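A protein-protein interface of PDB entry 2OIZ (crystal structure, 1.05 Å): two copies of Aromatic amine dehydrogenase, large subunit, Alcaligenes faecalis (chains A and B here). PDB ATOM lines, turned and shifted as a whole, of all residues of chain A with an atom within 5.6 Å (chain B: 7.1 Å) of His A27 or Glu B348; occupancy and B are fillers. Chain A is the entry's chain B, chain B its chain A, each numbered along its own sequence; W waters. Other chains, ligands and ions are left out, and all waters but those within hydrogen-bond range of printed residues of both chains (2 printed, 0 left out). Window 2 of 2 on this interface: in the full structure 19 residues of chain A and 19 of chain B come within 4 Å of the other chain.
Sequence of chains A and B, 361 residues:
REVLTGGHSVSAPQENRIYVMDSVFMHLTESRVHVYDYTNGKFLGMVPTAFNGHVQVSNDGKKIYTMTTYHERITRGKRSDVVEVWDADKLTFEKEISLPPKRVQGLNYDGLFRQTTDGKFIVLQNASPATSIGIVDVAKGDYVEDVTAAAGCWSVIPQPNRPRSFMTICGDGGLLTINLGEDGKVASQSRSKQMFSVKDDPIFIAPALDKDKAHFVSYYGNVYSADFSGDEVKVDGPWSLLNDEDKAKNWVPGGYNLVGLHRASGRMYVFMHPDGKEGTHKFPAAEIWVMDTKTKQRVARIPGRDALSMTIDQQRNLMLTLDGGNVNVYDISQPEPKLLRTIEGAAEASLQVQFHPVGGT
A ring nitrogen (NE2) of His A27 lies within hydrogen-bond range of the side-chain carboxylate (OE2) of Glu B348 (2.6 Å).
The backbone NH (N) of Leu A28 sits at hydrogen-bond distance from the side-chain carboxylate (OE1) of Glu B30 (3.3 Å).
A ring nitrogen (ND1) of His B27 is in hydrogen-bond range of the side-chain carboxylate of Glu A30 (2.8 Å).
ND1 of His A27 sits at hydrogen-bond distance from OE2 of Glu B30, 2.7 Å away.
OE1 of Glu B30 lies within hydrogen-bond range of OG1 of Thr A29, at 2.6 Å.
OG1 of Thr B29 sits at hydrogen-bond distance from OE1 of Glu A30 (2.6 Å).
The side-chain carboxylate of Asp B22 sits at hydrogen-bond distance from the backbone NH of Glu B348 (2.8 Å).
The backbone NH (N) of Asp B22 sits at hydrogen-bond distance from the backbone carbonyl oxygen (O) of Arg B32.
The side-chain carboxylate (OD1) of Asp B22 sits at hydrogen-bond distance from the backbone NH (N) of Val B24.
NH2 of Arg B32 lies within salt-bridge range of OE2 of Glu B30 (2.8 Å).
Among the printed residues, merely in contact across the chains: Val A24 with His B27 (3.4 Å), Met A26 with Glu B30 (3.7 Å), His A27 with Val B24 (3.5 Å), His A27 with Arg B32 (3.7 Å) and Glu A30 with Met B26 (3.7 Å).
Of the printed residues of chain B, Val A24 touches His B27 (3.4 Å).
Of the printed residues of chain B, His A27 touches Val B24 (3.5 Å), Glu B30 (2.7 Å), Arg B32 (3.7 Å) and Glu B348 (2.6 Å).
Of the printed residues of chain A, Glu B30 touches Met A26, His A27, Leu A28 and Thr A29.
Glu B348 touches one residue of chain A.
Hydrophobic or aromatic side chains of chain A that line the printed part of chain B: Val A24 and His A27.
Along chain A the printed residues that touch a printed residue of chain B span positions 24 to 30.
Of the 20 printed residues of chain B, 7 touch a printed residue of chain A.
Among the printed residues, 11 pairs touch across the chains.
Val A24 touches His B27, and with the chains exchanged His A27 touches Val B24.
Met A26 touches Glu B30, and with the chains exchanged Glu A30 touches Met B26.
His A27 touches Glu B30, and with the chains exchanged Glu A30 touches His B27.
Thr A29 touches Glu B30, and with the chains exchanged Glu A30 touches Thr B29.
8 positions are printed for both chains.
Water W2 lies within hydrogen-bond range of O of Thr B29 (2.7 Å) and OG1 of Thr A29 (2.8 Å).
Water W1 bridges O of Thr A29 (2.7 Å) and OG1 of Thr B29 (2.8 Å).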
ATOM      1  N   SER A  23      12.852 -27.504  14.738  1.00  0.00           N
ATOM      2  CA  SER A  23      12.390 -27.153  13.390  1.00  0.00           C
ATOM      3  C   SER A  23      13.390 -26.309  12.634  1.00  0.00           C
ATOM      4  O   SER A  23      13.407 -26.343  11.409  1.00  0.00           O
ATOM      5  CB  SER A  23      11.042 -26.436  13.417  1.00  0.00           C
ATOM      6  OG  SER A  23      11.132 -25.090  13.855  1.00  0.00           O
ATOM      7  N   VAL A  24      14.192 -25.507  13.353  1.00  0.00           N
ATOM      8  CA  VAL A  24      15.098 -24.568  12.683  1.00  0.00           C
ATOM      9  C   VAL A  24      14.288 -23.789  11.626  1.00  0.00           C
ATOM     10  O   VAL A  24      14.639 -23.730  10.452  1.00  0.00           O
ATOM     11  CB  VAL A  24      16.348 -25.238  12.073  1.00  0.00           C
ATOM     12  CG1 VAL A  24      17.380 -24.158  11.704  1.00  0.00           C
ATOM     13  CG2 VAL A  24      16.957 -26.245  12.993  1.00  0.00           C
ATOM     14  N   PHE A  25      13.207 -23.150  12.052  1.00  0.00           N
ATOM     15  CA  PHE A  25      12.311 -22.514  11.103  1.00  0.00           C
ATOM     16  C   PHE A  25      13.031 -21.513  10.194  1.00  0.00           C
ATOM     17  O   PHE A  25      12.644 -21.338   9.022  1.00  0.00           O
ATOM     18  CB  PHE A  25      11.144 -21.851  11.855  1.00  0.00           C
ATOM     19  CG  PHE A  25      10.005 -21.457  11.008  1.00  0.00           C
ATOM     20  CD1 PHE A  25       9.084 -22.383  10.520  1.00  0.00           C
ATOM     21  CD2 PHE A  25       9.825 -20.137  10.669  1.00  0.00           C
ATOM     22  CE1 PHE A  25       8.018 -21.990   9.706  1.00  0.00           C
ATOM     23  CE2 PHE A  25       8.789 -19.735   9.898  1.00  0.00           C
ATOM     24  CZ  PHE A  25       7.875 -20.637   9.405  1.00  0.00           C
ATOM     25  N   MET A  26      14.044 -20.817  10.706  1.00  0.00           N
ATOM     26  CA  MET A  26      14.792 -19.870   9.865  1.00  0.00           C
ATOM     27  C   MET A  26      15.526 -20.546   8.699  1.00  0.00           C
ATOM     28  O   MET A  26      15.870 -19.888   7.707  1.00  0.00           O
ATOM     29  CB  MET A  26      15.793 -19.080  10.681  1.00  0.00           C
ATOM     30  CG  MET A  26      15.157 -18.091  11.651  1.00  0.00           C
ATOM     31  SD  MET A  26      14.506 -16.643  10.818  1.00  0.00           S
ATOM     32  CE  MET A  26      16.068 -15.864  10.284  1.00  0.00           C
ATOM     33  N   HIS A  27      15.793 -21.846   8.866  1.00  0.00           N
ATOM     34  CA  HIS A  27      16.450 -22.670   7.839  1.00  0.00           C
ATOM     35  C   HIS A  27      15.785 -24.041   7.850  1.00  0.00           C
ATOM     36  O   HIS A  27      16.421 -25.053   8.152  1.00  0.00           O
ATOM     37  CB  HIS A  27      17.957 -22.752   8.075  1.00  0.00           C
ATOM     38  CG  HIS A  27      18.567 -21.410   8.006  1.00  0.00           C
ATOM     39  ND1 HIS A  27      18.655 -20.706   6.818  1.00  0.00           N
ATOM     40  CD2 HIS A  27      19.045 -20.610   8.973  1.00  0.00           C
ATOM     41  CE1 HIS A  27      19.148 -19.497   7.083  1.00  0.00           C
ATOM     42  NE2 HIS A  27      19.381 -19.414   8.386  1.00  0.00           N
ATOM     43  N   LEU A  28      14.483 -24.073   7.520  1.00  0.00           N
ATOM     44  CA  LEU A  28      13.618 -25.219   7.783  1.00  0.00           C
ATOM     45  C   LEU A  28      13.984 -26.452   7.005  1.00  0.00           C
ATOM     46  O   LEU A  28      13.519 -27.554   7.342  1.00  0.00           O
ATOM     47  CB  LEU A  28      12.159 -24.781   7.526  1.00  0.00           C
ATOM     48  CG  LEU A  28      11.020 -25.737   7.856  1.00  0.00           C
ATOM     49  CD1 LEU A  28      11.047 -26.218   9.303  1.00  0.00           C
ATOM     50  CD2 LEU A  28       9.686 -25.054   7.541  1.00  0.00           C
ATOM     51  N   THR A  29      14.793 -26.315   5.935  1.00  0.00           N
ATOM     52  CA  THR A  29      15.302 -27.482   5.229  1.00  0.00           C
ATOM     53  C   THR A  29      16.393 -28.236   5.991  1.00  0.00           C
ATOM     54  O   THR A  29      16.796 -29.287   5.525  1.00  0.00           O
ATOM     55  CB  THR A  29      15.828 -27.165   3.814  1.00  0.00           C
ATOM     56  OG1 THR A  29      16.987 -26.343   3.927  1.00  0.00           O
ATOM     57  CG2 THR A  29      14.756 -26.561   2.926  1.00  0.00           C
ATOM     58  N   GLU A  30      16.843 -27.715   7.145  1.00  0.00           N
ATOM     59  CA  GLU A  30      17.874 -28.361   7.970  1.00  0.00           C
ATOM     60  C   GLU A  30      17.385 -28.567   9.398  1.00  0.00           C
ATOM     61  O   GLU A  30      18.130 -28.464  10.351  1.00  0.00           O
ATOM     62  CB  GLU A  30      19.208 -27.622   7.870  1.00  0.00           C
ATOM     63  CG  GLU A  30      20.370 -28.593   8.147  1.00  0.00           C
ATOM     64  CD  GLU A  30      21.695 -27.897   8.349  1.00  0.00           C
ATOM     65  OE1 GLU A  30      22.422 -27.634   7.373  1.00  0.00           O
ATOM     66  OE2 GLU A  30      22.018 -27.601   9.533  1.00  0.00           O
ATOM     67  N   SER A  31      16.113 -28.933   9.518  1.00  0.00           N
ATOM     68  CA  SER A  31      15.566 -29.341  10.785  1.00  0.00           C
ATOM     69  C   SER A  31      16.306 -30.586  11.280  1.00  0.00           C
ATOM     70  O   SER A  31      16.916 -31.329  10.500  1.00  0.00           O
ATOM     71  CB  SER A  31      14.050 -29.624  10.672  1.00  0.00           C
ATOM     72  OG  SER A  31      13.759 -30.820   9.945  1.00  0.00           O
ATOM     73  N   VAL B  20      25.250 -10.849  -1.519  1.00  0.00           N
ATOM     74  CA  VAL B  20      25.879 -11.240  -0.277  1.00  0.00           C
ATOM     75  C   VAL B  20      25.758 -12.757  -0.169  1.00  0.00           C
ATOM     76  O   VAL B  20      24.655 -13.284  -0.067  1.00  0.00           O
ATOM     77  CB  VAL B  20      25.194 -10.535   0.926  1.00  0.00           C
ATOM     78  CG1 VAL B  20      25.910 -10.920   2.248  1.00  0.00           C
ATOM     79  CG2 VAL B  20      25.223  -9.018   0.754  1.00  0.00           C
ATOM     80  N   ASP B  22      25.665 -15.831   1.626  1.00  0.00           N
ATOM     81  CA  ASP B  22      25.491 -16.248   3.021  1.00  0.00           C
ATOM     82  C   ASP B  22      25.749 -17.744   3.109  1.00  0.00           C
ATOM     83  O   ASP B  22      24.940 -18.579   2.676  1.00  0.00           O
ATOM     84  CB  ASP B  22      24.092 -15.916   3.517  1.00  0.00           C
ATOM     85  CG  ASP B  22      24.017 -15.956   5.048  1.00  0.00           C
ATOM     86  OD1 ASP B  22      25.007 -16.425   5.692  1.00  0.00           O
ATOM     87  OD2 ASP B  22      22.977 -15.513   5.597  1.00  0.00           O
ATOM     88  N   SER B  23      26.895 -18.100   3.651  1.00  0.00           N
ATOM     89  CA  SER B  23      27.183 -19.523   3.876  1.00  0.00           C
ATOM     90  C   SER B  23      26.229 -20.182   4.854  1.00  0.00           C
ATOM     91  O   SER B  23      26.035 -21.399   4.791  1.00  0.00           O
ATOM     92  CB  SER B  23      28.628 -19.737   4.369  1.00  0.00           C
ATOM     93  OG  SER B  23      28.785 -19.397   5.726  1.00  0.00           O
ATOM     94  N   VAL B  24      25.663 -19.408   5.791  1.00  0.00           N
ATOM     95  CA  VAL B  24      24.814 -20.009   6.834  1.00  0.00           C
ATOM     96  C   VAL B  24      25.542 -21.212   7.420  1.00  0.00           C
ATOM     97  O   VAL B  24      25.019 -22.326   7.498  1.00  0.00           O
ATOM     98  CB  VAL B  24      23.399 -20.400   6.342  1.00  0.00           C
ATOM     99  CG1 VAL B  24      22.500 -20.643   7.568  1.00  0.00           C
ATOM    100  CG2 VAL B  24      22.790 -19.309   5.505  1.00  0.00           C
ATOM    101  N   PHE B  25      26.758 -20.993   7.890  1.00  0.00           N
ATOM    102  CA  PHE B  25      27.596 -22.099   8.353  1.00  0.00           C
ATOM    103  C   PHE B  25      26.923 -22.949   9.459  1.00  0.00           C
ATOM    104  O   PHE B  25      27.138 -24.164   9.517  1.00  0.00           O
ATOM    105  CB  PHE B  25      28.950 -21.552   8.828  1.00  0.00           C
ATOM    106  CG  PHE B  25      30.007 -22.600   9.010  1.00  0.00           C
ATOM    107  CD1 PHE B  25      30.672 -23.146   7.908  1.00  0.00           C
ATOM    108  CD2 PHE B  25      30.349 -23.047  10.271  1.00  0.00           C
ATOM    109  CE1 PHE B  25      31.642 -24.118   8.065  1.00  0.00           C
ATOM    110  CE2 PHE B  25      31.330 -24.020  10.434  1.00  0.00           C
ATOM    111  CZ  PHE B  25      31.967 -24.559   9.337  1.00  0.00           C
ATOM    112  N   MET B  26      26.101 -22.331  10.319  1.00  0.00           N
ATOM    113  CA  MET B  26      25.393 -23.108  11.330  1.00  0.00           C
ATOM    114  C   MET B  26      24.398 -24.110  10.737  1.00  0.00           C
ATOM    115  O   MET B  26      23.985 -25.076  11.375  1.00  0.00           O
ATOM    116  CB  MET B  26      24.633 -22.209  12.294  1.00  0.00           C
ATOM    117  CG  MET B  26      25.550 -21.396  13.189  1.00  0.00           C
ATOM    118  SD  MET B  26      26.271 -22.382  14.501  1.00  0.00           S
ATOM    119  CE  MET B  26      24.812 -22.677  15.529  1.00  0.00           C
ATOM    120  N   HIS B  27      23.968 -23.851   9.503  1.00  0.00           N
ATOM    121  CA  HIS B  27      23.050 -24.696   8.734  1.00  0.00           C
ATOM    122  C   HIS B  27      23.499 -24.689   7.282  1.00  0.00           C
ATOM    123  O   HIS B  27      22.759 -24.251   6.409  1.00  0.00           O
ATOM    124  CB  HIS B  27      21.586 -24.237   8.910  1.00  0.00           C
ATOM    125  CG  HIS B  27      21.164 -24.292  10.317  1.00  0.00           C
ATOM    126  ND1 HIS B  27      21.017 -25.484  10.994  1.00  0.00           N
ATOM    127  CD2 HIS B  27      20.977 -23.315  11.227  1.00  0.00           C
ATOM    128  CE1 HIS B  27      20.773 -25.233  12.274  1.00  0.00           C
ATOM    129  NE2 HIS B  27      20.740 -23.927  12.443  1.00  0.00           N
ATOM    130  N   THR B  29      23.809 -26.574   4.801  1.00  0.00           N
ATOM    131  CA  THR B  29      23.008 -27.130   3.707  1.00  0.00           C
ATOM    132  C   THR B  29      21.966 -26.163   3.169  1.00  0.00           C
ATOM    133  O   THR B  29      21.323 -26.489   2.181  1.00  0.00           O
ATOM    134  CB  THR B  29      22.317 -28.439   4.058  1.00  0.00           C
ATOM    135  OG1 THR B  29      21.319 -28.241   5.068  1.00  0.00           O
ATOM    136  CG2 THR B  29      23.316 -29.539   4.467  1.00  0.00           C
ATOM    137  N   GLU B  30      21.806 -24.998   3.805  1.00  0.00           N
ATOM    138  CA  GLU B  30      20.832 -23.987   3.377  1.00  0.00           C
ATOM    139  C   GLU B  30      21.497 -22.634   3.131  1.00  0.00           C
ATOM    140  O   GLU B  30      20.914 -21.566   3.359  1.00  0.00           O
ATOM    141  CB  GLU B  30      19.609 -23.878   4.301  1.00  0.00           C
ATOM    142  CG  GLU B  30      18.369 -23.410   3.537  1.00  0.00           C
ATOM    143  CD  GLU B  30      17.239 -23.058   4.464  1.00  0.00           C
ATOM    144  OE1 GLU B  30      16.393 -23.948   4.779  1.00  0.00           O
ATOM    145  OE2 GLU B  30      17.155 -21.862   4.831  1.00  0.00           O
ATOM    146  N   SER B  31      22.703 -22.691   2.564  1.00  0.00           N
ATOM    147  CA  SER B  31      23.372 -21.478   2.104  1.00  0.00           C
ATOM    148  C   SER B  31      22.518 -20.806   1.024  1.00  0.00           C
ATOM    149  O   SER B  31      21.706 -21.447   0.359  1.00  0.00           O
ATOM    150  CB  SER B  31      24.764 -21.802   1.589  1.00  0.00           C
ATOM    151  OG  SER B  31      24.749 -22.523   0.348  1.00  0.00           O
ATOM    152  N   ARG B  32      22.719 -19.508   0.853  1.00  0.00           N
ATOM    153  CA  ARG B  32      21.988 -18.762  -0.172  1.00  0.00           C
ATOM    154  C   ARG B  32      22.673 -17.469  -0.456  1.00  0.00           C
ATOM    155  O   ARG B  32      23.492 -16.985   0.326  1.00  0.00           O
ATOM    156  CB  ARG B  32      20.547 -18.462   0.286  1.00  0.00           C
ATOM    157  CG  ARG B  32      20.399 -17.428   1.389  1.00  0.00           C
ATOM    158  CD  ARG B  32      20.558 -17.960   2.823  1.00  0.00           C
ATOM    159  NE  ARG B  32      19.467 -18.858   3.218  1.00  0.00           N
ATOM    160  CZ  ARG B  32      18.211 -18.424   3.455  1.00  0.00           C
ATOM    161  NH1 ARG B  32      17.942 -17.146   3.475  1.00  0.00           N
ATOM    162  NH2 ARG B  32      17.267 -19.303   3.730  1.00  0.00           N
ATOM    163  N   HIS B  34      21.913 -13.500  -0.903  1.00  0.00           N
ATOM    164  CA  HIS B  34      20.963 -12.439  -0.658  1.00  0.00           C
ATOM    165  C   HIS B  34      21.270 -11.261  -1.582  1.00  0.00           C
ATOM    166  O   HIS B  34      22.410 -10.826  -1.653  1.00  0.00           O
ATOM    167  CB  HIS B  34      21.020 -11.973   0.821  1.00  0.00           C
ATOM    168  CG  HIS B  34      20.614 -12.983   1.846  1.00  0.00           C
ATOM    169  ND1 HIS B  34      19.716 -14.030   1.713  1.00  0.00           N
ATOM    170  CD2 HIS B  34      21.031 -13.024   3.133  1.00  0.00           C
ATOM    171  CE1 HIS B  34      19.608 -14.672   2.883  1.00  0.00           C
ATOM    172  NE2 HIS B  34      20.404 -14.075   3.740  1.00  0.00           N
ATOM    173  N   GLY B 324      30.888 -10.193   8.268  1.00  0.00           N
ATOM    174  CA  GLY B 324      30.238 -11.477   8.453  1.00  0.00           C
ATOM    175  C   GLY B 324      28.721 -11.395   8.425  1.00  0.00           C
ATOM    176  O   GLY B 324      28.042 -12.346   8.022  1.00  0.00           O
ATOM    177  N   GLY B 325      28.198 -10.254   8.874  1.00  0.00           N
ATOM    178  CA  GLY B 325      26.762 -10.035   8.945  1.00  0.00           C
ATOM    179  C   GLY B 325      26.260  -8.734   8.343  1.00  0.00           C
ATOM    180  O   GLY B 325      25.126  -8.660   7.852  1.00  0.00           O
ATOM    181  N   GLY B 345      22.456  -6.936   9.149  1.00  0.00           N
ATOM    182  CA  GLY B 345      21.766  -8.200   9.009  1.00  0.00           C
ATOM    183  C   GLY B 345      21.583  -8.650   7.574  1.00  0.00           C
ATOM    184  O   GLY B 345      20.606  -9.337   7.235  1.00  0.00           O
ATOM    185  N   ALA B 346      22.564  -8.324   6.754  1.00  0.00           N
ATOM    186  CA  ALA B 346      22.571  -8.760   5.374  1.00  0.00           C
ATOM    187  C   ALA B 346      22.826 -10.265   5.235  1.00  0.00           C
ATOM    188  O   ALA B 346      22.488 -10.843   4.189  1.00  0.00           O
ATOM    189  CB  ALA B 346      23.618  -8.000   4.612  1.00  0.00           C
ATOM    190  N   ALA B 347      23.448 -10.875   6.242  1.00  0.00           N
ATOM    191  CA  ALA B 347      23.703 -12.297   6.225  1.00  0.00           C
ATOM    192  C   ALA B 347      23.921 -12.735   7.656  1.00  0.00           C
ATOM    193  O   ALA B 347      24.192 -11.915   8.527  1.00  0.00           O
ATOM    194  CB  ALA B 347      24.969 -12.588   5.433  1.00  0.00           C
ATOM    195  N   GLU B 348      23.837 -14.042   7.862  1.00  0.00           N
ATOM    196  CA  GLU B 348      24.257 -14.653   9.118  1.00  0.00           C
ATOM    197  C   GLU B 348      25.738 -14.992   9.146  1.00  0.00           C
ATOM    198  O   GLU B 348      26.376 -14.831  10.198  1.00  0.00           O
ATOM    199  CB  GLU B 348      23.404 -15.854   9.417  1.00  0.00           C
ATOM    200  CG  GLU B 348      21.984 -15.480   9.749  1.00  0.00           C
ATOM    201  CD  GLU B 348      21.185 -16.704  10.006  1.00  0.00           C
ATOM    202  OE1 GLU B 348      21.203 -17.242  11.147  1.00  0.00           O
ATOM    203  OE2 GLU B 348      20.670 -17.265   9.086  1.00  0.00           O
ATOM    204  N   ALA B 349      26.297 -15.457   8.039  1.00  0.00           N
ATOM    205  CA  ALA B 349      27.683 -15.877   7.983  1.00  0.00           C
ATOM    206  C   ALA B 349      28.208 -15.730   6.562  1.00  0.00           C
ATOM    207  O   ALA B 349      28.335 -16.704   5.819  1.00  0.00           O
ATOM    208  CB  ALA B 349      27.834 -17.304   8.480  1.00  0.00           C
ATOM    209  N   SER B 350      28.513 -14.494   6.179  1.00  0.00           N
ATOM    210  CA  SER B 350      29.036 -14.220   4.855  1.00  0.00           C
ATOM    211  C   SER B 350      30.449 -13.694   4.914  1.00  0.00           C
ATOM    212  O   SER B 350      30.764 -12.805   5.683  1.00  0.00           O
ATOM    213  CB  SER B 350      28.190 -13.169   4.136  1.00  0.00           C
ATOM    214  OG  SER B 350      28.718 -12.923   2.845  1.00  0.00           O
HETATM  215  O   HOH W   1      19.343 -30.150   4.951  1.00  0.00           O
HETATM  216  O   HOH W   2      18.626 -26.614   1.713  1.00  0.00           O
